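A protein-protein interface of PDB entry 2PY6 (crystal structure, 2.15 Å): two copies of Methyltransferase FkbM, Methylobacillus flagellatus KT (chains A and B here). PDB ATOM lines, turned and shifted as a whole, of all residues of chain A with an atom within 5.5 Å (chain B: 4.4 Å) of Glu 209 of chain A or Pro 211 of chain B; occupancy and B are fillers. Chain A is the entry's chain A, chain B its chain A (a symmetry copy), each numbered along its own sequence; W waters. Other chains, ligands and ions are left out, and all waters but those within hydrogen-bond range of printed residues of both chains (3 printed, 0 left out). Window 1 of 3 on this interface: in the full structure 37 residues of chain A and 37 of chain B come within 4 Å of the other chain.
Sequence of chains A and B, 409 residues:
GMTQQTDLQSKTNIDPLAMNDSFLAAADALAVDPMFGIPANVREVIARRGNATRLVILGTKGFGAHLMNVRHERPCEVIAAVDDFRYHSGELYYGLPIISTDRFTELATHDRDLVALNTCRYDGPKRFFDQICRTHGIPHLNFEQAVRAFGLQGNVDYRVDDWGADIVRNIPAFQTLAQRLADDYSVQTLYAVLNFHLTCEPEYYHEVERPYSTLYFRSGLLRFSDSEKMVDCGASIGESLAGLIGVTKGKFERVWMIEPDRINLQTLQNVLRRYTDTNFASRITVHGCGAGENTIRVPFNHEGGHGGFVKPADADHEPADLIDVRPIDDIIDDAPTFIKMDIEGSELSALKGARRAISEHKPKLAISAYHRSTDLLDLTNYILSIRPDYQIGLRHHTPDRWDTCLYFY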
ATOM      1  N   TYR A 185     -12.841 -18.801 -24.002  1.00  0.00           N
ATOM      2  CA  TYR A 185     -14.175 -18.666 -24.587  1.00  0.00           C
ATOM      3  C   TYR A 185     -14.670 -19.963 -25.312  1.00  0.00           C
ATOM      4  O   TYR A 185     -15.861 -20.302 -25.330  1.00  0.00           O
ATOM      5  CB  TYR A 185     -14.202 -17.389 -25.479  1.00  0.00           C
ATOM      6  CG  TYR A 185     -15.558 -17.034 -26.059  1.00  0.00           C
ATOM      7  CD1 TYR A 185     -16.737 -17.242 -25.339  1.00  0.00           C
ATOM      8  CD2 TYR A 185     -15.657 -16.409 -27.285  1.00  0.00           C
ATOM      9  CE1 TYR A 185     -17.987 -16.887 -25.862  1.00  0.00           C
ATOM     10  CE2 TYR A 185     -16.901 -16.051 -27.809  1.00  0.00           C
ATOM     11  CZ  TYR A 185     -18.065 -16.297 -27.083  1.00  0.00           C
ATOM     12  OH  TYR A 185     -19.290 -15.921 -27.586  1.00  0.00           O
ATOM     13  N   TYR A 205     -26.952 -21.783 -24.721  1.00  0.00           N
ATOM     14  CA  TYR A 205     -26.457 -21.290 -26.019  1.00  0.00           C
ATOM     15  C   TYR A 205     -26.397 -19.782 -26.038  1.00  0.00           C
ATOM     16  O   TYR A 205     -25.454 -19.214 -26.561  1.00  0.00           O
ATOM     17  CB  TYR A 205     -27.407 -21.617 -27.213  1.00  0.00           C
ATOM     18  CG  TYR A 205     -27.362 -23.034 -27.651  1.00  0.00           C
ATOM     19  CD1 TYR A 205     -26.166 -23.580 -28.106  1.00  0.00           C
ATOM     20  CD2 TYR A 205     -28.505 -23.834 -27.669  1.00  0.00           C
ATOM     21  CE1 TYR A 205     -26.078 -24.901 -28.545  1.00  0.00           C
ATOM     22  CE2 TYR A 205     -28.430 -25.156 -28.120  1.00  0.00           C
ATOM     23  CZ  TYR A 205     -27.197 -25.688 -28.557  1.00  0.00           C
ATOM     24  OH  TYR A 205     -27.051 -27.009 -28.995  1.00  0.00           O
ATOM     25  N   HIS A 206     -27.443 -19.146 -25.508  1.00  0.00           N
ATOM     26  CA  HIS A 206     -27.537 -17.709 -25.556  1.00  0.00           C
ATOM     27  C   HIS A 206     -26.398 -16.973 -24.865  1.00  0.00           C
ATOM     28  O   HIS A 206     -26.032 -15.899 -25.310  1.00  0.00           O
ATOM     29  CB  HIS A 206     -28.906 -17.201 -25.079  1.00  0.00           C
ATOM     30  CG  HIS A 206     -30.064 -17.803 -25.798  1.00  0.00           C
ATOM     31  ND1 HIS A 206     -30.055 -18.039 -27.155  1.00  0.00           N
ATOM     32  CD2 HIS A 206     -31.299 -18.150 -25.366  1.00  0.00           C
ATOM     33  CE1 HIS A 206     -31.220 -18.541 -27.520  1.00  0.00           C
ATOM     34  NE2 HIS A 206     -31.995 -18.614 -26.452  1.00  0.00           N
ATOM     35  N   GLU A 207     -25.812 -17.571 -23.829  1.00  0.00           N
ATOM     36  CA  GLU A 207     -24.716 -16.952 -23.095  1.00  0.00           C
ATOM     37  C   GLU A 207     -23.444 -16.857 -23.915  1.00  0.00           C
ATOM     38  O   GLU A 207     -22.607 -16.004 -23.662  1.00  0.00           O
ATOM     39  CB  GLU A 207     -24.373 -17.766 -21.814  1.00  0.00           C
ATOM     40  CG  GLU A 207     -25.387 -17.746 -20.714  1.00  0.00           C
ATOM     41  CD  GLU A 207     -25.531 -16.433 -19.943  1.00  0.00           C
ATOM     42  OE1 GLU A 207     -24.873 -15.396 -20.200  1.00  0.00           O
ATOM     43  OE2 GLU A 207     -26.378 -16.448 -19.057  1.00  0.00           O
ATOM     44  N   VAL A 208     -23.287 -17.745 -24.882  1.00  0.00           N
ATOM     45  CA  VAL A 208     -22.055 -17.808 -25.673  1.00  0.00           C
ATOM     46  C   VAL A 208     -22.193 -17.550 -27.193  1.00  0.00           C
ATOM     47  O   VAL A 208     -21.208 -17.318 -27.860  1.00  0.00           O
ATOM     48  CB  VAL A 208     -21.373 -19.200 -25.494  1.00  0.00           C
ATOM     49  CG1 VAL A 208     -21.018 -19.441 -24.031  1.00  0.00           C
ATOM     50  CG2 VAL A 208     -22.257 -20.361 -26.046  1.00  0.00           C
ATOM     51  N   GLU A 209     -23.405 -17.631 -27.718  1.00  0.00           N
ATOM     52  CA  GLU A 209     -23.639 -17.534 -29.141  1.00  0.00           C
ATOM     53  C   GLU A 209     -23.089 -16.263 -29.812  1.00  0.00           C
ATOM     54  O   GLU A 209     -23.050 -15.190 -29.233  1.00  0.00           O
ATOM     55  CB  GLU A 209     -25.137 -17.626 -29.450  1.00  0.00           C
ATOM     56  CG  GLU A 209     -25.906 -16.309 -29.261  1.00  0.00           C
ATOM     57  CD  GLU A 209     -27.399 -16.408 -29.555  1.00  0.00           C
ATOM     58  OE1 GLU A 209     -28.112 -16.856 -28.688  1.00  0.00           O
ATOM     59  OE2 GLU A 209     -27.859 -15.994 -30.637  1.00  0.00           O
ATOM     60  N   ARG A 210     -22.710 -16.428 -31.071  1.00  0.00           N
ATOM     61  CA  ARG A 210     -22.262 -15.353 -31.926  1.00  0.00           C
ATOM     62  C   ARG A 210     -23.233 -15.334 -33.082  1.00  0.00           C
ATOM     63  O   ARG A 210     -23.997 -16.294 -33.250  1.00  0.00           O
ATOM     64  CB  ARG A 210     -20.815 -15.605 -32.331  1.00  0.00           C
ATOM     65  CG  ARG A 210     -19.929 -15.703 -31.060  1.00  0.00           C
ATOM     66  CD  ARG A 210     -18.574 -15.081 -31.128  1.00  0.00           C
ATOM     67  NE  ARG A 210     -18.608 -13.848 -31.905  1.00  0.00           N
ATOM     68  CZ  ARG A 210     -17.948 -13.640 -33.027  1.00  0.00           C
ATOM     69  NH1 ARG A 210     -17.011 -14.489 -33.463  1.00  0.00           N
ATOM     70  NH2 ARG A 210     -18.144 -12.515 -33.686  1.00  0.00           N
ATOM     71  N   PRO A 211     -23.300 -14.219 -33.831  1.00  0.00           N
ATOM     72  CA  PRO A 211     -24.217 -14.202 -34.963  1.00  0.00           C
ATOM     73  C   PRO A 211     -23.885 -15.214 -36.070  1.00  0.00           C
ATOM     74  O   PRO A 211     -22.710 -15.618 -36.258  1.00  0.00           O
ATOM     75  CB  PRO A 211     -24.052 -12.780 -35.527  1.00  0.00           C
ATOM     76  CG  PRO A 211     -23.493 -11.984 -34.420  1.00  0.00           C
ATOM     77  CD  PRO A 211     -22.590 -12.943 -33.700  1.00  0.00           C
ATOM     78  N   HIS A 396     -20.212 -21.050 -31.215  1.00  0.00           N
ATOM     79  CA  HIS A 396     -21.569 -21.412 -31.534  1.00  0.00           C
ATOM     80  C   HIS A 396     -22.189 -20.218 -32.243  1.00  0.00           C
ATOM     81  O   HIS A 396     -22.229 -19.148 -31.675  1.00  0.00           O
ATOM     82  CB  HIS A 396     -22.361 -21.771 -30.290  1.00  0.00           C
ATOM     83  CG  HIS A 396     -23.757 -22.180 -30.614  1.00  0.00           C
ATOM     84  ND1 HIS A 396     -24.058 -23.430 -31.105  1.00  0.00           N
ATOM     85  CD2 HIS A 396     -24.912 -21.480 -30.634  1.00  0.00           C
ATOM     86  CE1 HIS A 396     -25.349 -23.499 -31.367  1.00  0.00           C
ATOM     87  NE2 HIS A 396     -25.891 -22.329 -31.097  1.00  0.00           N
ATOM     88  N   HIS A 397     -22.708 -20.410 -33.458  1.00  0.00           N
ATOM     89  CA  HIS A 397     -23.145 -19.283 -34.296  1.00  0.00           C
ATOM     90  C   HIS A 397     -24.642 -19.058 -34.654  1.00  0.00           C
ATOM     91  O   HIS A 397     -24.923 -18.357 -35.633  1.00  0.00           O
ATOM     92  CB  HIS A 397     -22.387 -19.309 -35.607  1.00  0.00           C
ATOM     93  CG  HIS A 397     -20.917 -19.157 -35.480  1.00  0.00           C
ATOM     94  ND1 HIS A 397     -20.289 -17.934 -35.558  1.00  0.00           N
ATOM     95  CD2 HIS A 397     -19.932 -20.080 -35.328  1.00  0.00           C
ATOM     96  CE1 HIS A 397     -18.977 -18.106 -35.443  1.00  0.00           C
ATOM     97  NE2 HIS A 397     -18.734 -19.400 -35.323  1.00  0.00           N
ATOM     98  N   THR A 398     -25.577 -19.636 -33.914  1.00  0.00           N
ATOM     99  CA  THR A 398     -26.992 -19.316 -34.092  1.00  0.00           C
ATOM    100  C   THR A 398     -27.628 -19.183 -32.703  1.00  0.00           C
ATOM    101  O   THR A 398     -27.028 -19.585 -31.714  1.00  0.00           O
ATOM    102  CB  THR A 398     -27.803 -20.408 -34.902  1.00  0.00           C
ATOM    103  OG1 THR A 398     -27.826 -21.652 -34.185  1.00  0.00           O
ATOM    104  CG2 THR A 398     -27.250 -20.624 -36.296  1.00  0.00           C
ATOM    105  N   PRO A 399     -28.829 -18.586 -32.624  1.00  0.00           N
ATOM    106  CA  PRO A 399     -29.595 -18.625 -31.375  1.00  0.00           C
ATOM    107  C   PRO A 399     -30.235 -20.004 -31.113  1.00  0.00           C
ATOM    108  O   PRO A 399     -30.920 -20.149 -30.127  1.00  0.00           O
ATOM    109  CB  PRO A 399     -30.724 -17.609 -31.592  1.00  0.00           C
ATOM    110  CG  PRO A 399     -30.491 -17.014 -32.927  1.00  0.00           C
ATOM    111  CD  PRO A 399     -29.510 -17.806 -33.674  1.00  0.00           C
ATOM    112  N   ARG B 210     -21.435  -9.969 -30.610  1.00  0.00           N
ATOM    113  CA  ARG B 210     -22.424 -10.910 -30.137  1.00  0.00           C
ATOM    114  C   ARG B 210     -23.751 -10.359 -30.603  1.00  0.00           C
ATOM    115  O   ARG B 210     -23.813  -9.195 -31.019  1.00  0.00           O
ATOM    116  CB  ARG B 210     -22.303 -11.047 -28.624  1.00  0.00           C
ATOM    117  CG  ARG B 210     -20.871 -11.522 -28.259  1.00  0.00           C
ATOM    118  CD  ARG B 210     -20.748 -12.511 -27.147  1.00  0.00           C
ATOM    119  NE  ARG B 210     -21.853 -13.462 -27.174  1.00  0.00           N
ATOM    120  CZ  ARG B 210     -22.749 -13.611 -26.219  1.00  0.00           C
ATOM    121  NH1 ARG B 210     -22.609 -13.029 -25.022  1.00  0.00           N
ATOM    122  NH2 ARG B 210     -23.759 -14.437 -26.411  1.00  0.00           N
ATOM    123  N   PRO B 211     -24.802 -11.197 -30.643  1.00  0.00           N
ATOM    124  CA  PRO B 211     -26.090 -10.667 -31.070  1.00  0.00           C
ATOM    125  C   PRO B 211     -26.677  -9.592 -30.143  1.00  0.00           C
ATOM    126  O   PRO B 211     -26.388  -9.552 -28.920  1.00  0.00           O
ATOM    127  CB  PRO B 211     -27.007 -11.903 -31.036  1.00  0.00           C
ATOM    128  CG  PRO B 211     -26.099 -13.062 -31.108  1.00  0.00           C
ATOM    129  CD  PRO B 211     -24.888 -12.627 -30.335  1.00  0.00           C
ATOM    130  N   TYR B 212     -27.467  -8.711 -30.741  1.00  0.00           N
ATOM    131  CA  TYR B 212     -28.232  -7.675 -30.023  1.00  0.00           C
ATOM    132  C   TYR B 212     -29.081  -8.300 -28.919  1.00  0.00           C
ATOM    133  O   TYR B 212     -29.116  -7.787 -27.784  1.00  0.00           O
ATOM    134  CB  TYR B 212     -29.044  -6.836 -31.037  1.00  0.00           C
ATOM    135  CG  TYR B 212     -29.897  -5.768 -30.404  1.00  0.00           C
ATOM    136  CD1 TYR B 212     -29.326  -4.621 -29.865  1.00  0.00           C
ATOM    137  CD2 TYR B 212     -31.275  -5.915 -30.337  1.00  0.00           C
ATOM    138  CE1 TYR B 212     -30.124  -3.629 -29.261  1.00  0.00           C
ATOM    139  CE2 TYR B 212     -32.082  -4.939 -29.737  1.00  0.00           C
ATOM    140  CZ  TYR B 212     -31.491  -3.800 -29.208  1.00  0.00           C
ATOM    141  OH  TYR B 212     -32.283  -2.836 -28.638  1.00  0.00           O
ATOM    142  N   SER B 213     -29.682  -9.446 -29.217  1.00  0.00           N
ATOM    143  CA  SER B 213     -30.511 -10.219 -28.251  1.00  0.00           C
ATOM    144  C   SER B 213     -29.828 -10.667 -26.956  1.00  0.00           C
ATOM    145  O   SER B 213     -30.486 -11.074 -26.003  1.00  0.00           O
ATOM    146  CB  SER B 213     -31.078 -11.471 -28.924  1.00  0.00           C
ATOM    147  OG  SER B 213     -30.056 -12.410 -29.244  1.00  0.00           O
ATOM    148  N   THR B 214     -28.506 -10.602 -26.908  1.00  0.00           N
ATOM    149  CA  THR B 214     -27.754 -11.004 -25.743  1.00  0.00           C
ATOM    150  C   THR B 214     -27.275  -9.829 -24.902  1.00  0.00           C
ATOM    151  O   THR B 214     -26.616 -10.028 -23.883  1.00  0.00           O
ATOM    152  CB  THR B 214     -26.530 -11.881 -26.197  1.00  0.00           C
ATOM    153  OG1 THR B 214     -25.590 -11.097 -26.938  1.00  0.00           O
ATOM    154  CG2 THR B 214     -27.005 -13.006 -27.043  1.00  0.00           C
ATOM    155  N   LEU B 215     -27.616  -8.602 -25.318  1.00  0.00           N
ATOM    156  CA  LEU B 215     -27.194  -7.418 -24.587  1.00  0.00           C
ATOM    157  C   LEU B 215     -27.753  -7.453 -23.168  1.00  0.00           C
ATOM    158  O   LEU B 215     -28.917  -7.710 -23.010  1.00  0.00           O
ATOM    159  CB  LEU B 215     -27.695  -6.163 -25.329  1.00  0.00           C
ATOM    160  CG  LEU B 215     -27.349  -4.749 -24.854  1.00  0.00           C
ATOM    161  CD1 LEU B 215     -25.866  -4.418 -24.872  1.00  0.00           C
ATOM    162  CD2 LEU B 215     -28.096  -3.813 -25.769  1.00  0.00           C
ATOM    163  N   HIS B 397     -22.330  -5.765 -28.853  1.00  0.00           N
ATOM    164  CA  HIS B 397     -23.570  -6.476 -29.200  1.00  0.00           C
ATOM    165  C   HIS B 397     -24.387  -6.128 -30.476  1.00  0.00           C
ATOM    166  O   HIS B 397     -25.575  -6.464 -30.535  1.00  0.00           O
ATOM    167  CB  HIS B 397     -24.534  -6.400 -28.035  1.00  0.00           C
ATOM    168  CG  HIS B 397     -24.054  -7.035 -26.784  1.00  0.00           C
ATOM    169  ND1 HIS B 397     -24.336  -8.343 -26.461  1.00  0.00           N
ATOM    170  CD2 HIS B 397     -23.345  -6.532 -25.740  1.00  0.00           C
ATOM    171  CE1 HIS B 397     -23.807  -8.628 -25.277  1.00  0.00           C
ATOM    172  NE2 HIS B 397     -23.219  -7.540 -24.809  1.00  0.00           N
HETATM  173  O   HOH W   1     -29.806 -13.912 -31.474  1.00  0.00           O
HETATM  174  O   HOH W   2     -19.901 -14.041 -24.347  1.00  0.00           O
HETATM  175  O   HOH W   3     -30.009 -14.664 -27.862  1.00  0.00           O
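The guanidinium group of Arg 210 of chain B lies within hydrogen-bond range of the backbone carbonyl oxygen of His 206 of chain A (2.9 Å). The backbone carbonyl oxygen of Glu 207 of chain A sits at hydrogen-bond distance from the guanidinium group of Arg 210 of chain B (3.3 Å). O of Glu 209 of chain A lies within hydrogen-bond range of NE of Arg 210 of chain B, at 2.9 Å.
A ring nitrogen (ND1) of His 397 of chain B lies within hydrogen-bond range of the side-chain hydroxyl of Thr 214 of chain B (3.1 Å). The side-chain hydroxyl (OG1) of Thr 214 of chain B lies within hydrogen-bond range of the backbone carbonyl oxygen (O) of Pro 211 of chain B (2.6 Å). The backbone carbonyl oxygen (O) of Pro 211 of chain B is in hydrogen-bond range of a ring nitrogen (ND1) of His 397 of chain B (3.4 Å). OE1 of Glu 209 of chain A is in hydrogen-bond range of ND1 of His 206 of chain A (2.7 Å).
Arg 210 of chain B touches Tyr 185 of chain A (NE to OH, 3.6 Å). His 206 of chain A touches Thr 214 of chain B. C of Val 208 of chain A touches NH2 of Arg 210 of chain B, 3.6 Å away. Glu 209 of chain A touches Pro 211 of chain B.
Printed residues of chain A within 4 Å of Arg 210 of chain B: Tyr 185, His 206, Glu 207, Val 208 and Glu 209. Printed residues of chain B within 4 Å of Glu 207 of chain A: Arg 210. Printed residues of chain A within 4 Å of Thr 214 of chain B: His 206 (3.5 Å). Of the printed residues of chain B, Tyr 185 of chain A touches Arg 210. Of the printed residues of chain B, Val 208 of chain A touches Arg 210. The nearest residue of chain B that does not touch Glu 209 of chain A is Thr 214 of chain B (4.1 Å). The nearest printed residue of chain B that does not touch Tyr 185 of chain A is Pro 211 of chain B (7.1 Å).
Printed residues of chain B that touch a printed residue of chain A: Arg 210, Pro 211 and Thr 214. Hydrophobic or aromatic side chains of chain B within 4 Å of the printed part of chain A: Pro 211. Along chain B the printed residues that touch a printed residue of chain A span positions 210 to 214. Hydrophobic or aromatic side chains of chain A that line the printed part of chain B: Tyr 185. Among the printed residues, no Asp or Glu carboxylate lies within 4 Å of a Lys or Arg side-chain nitrogen of the other chain.
Positions printed for both chains: 210, 211 and 397.
Water W3 lies within hydrogen-bond range of OG of Ser 213 of chain B, OE1 of Glu 209 of chain A and ND1 of His 206 of chain A. Water W1 bridges OG of Ser 213 of chain B (2.7 Å) and OE2 of Glu 209 of chain A (3.0 Å). Water W2 lies within hydrogen-bond range of the guanidinium group of Arg 210 of chain B (3.0 Å) and the backbone carbonyl oxygen of Glu 207 of chain A (3.4 Å).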
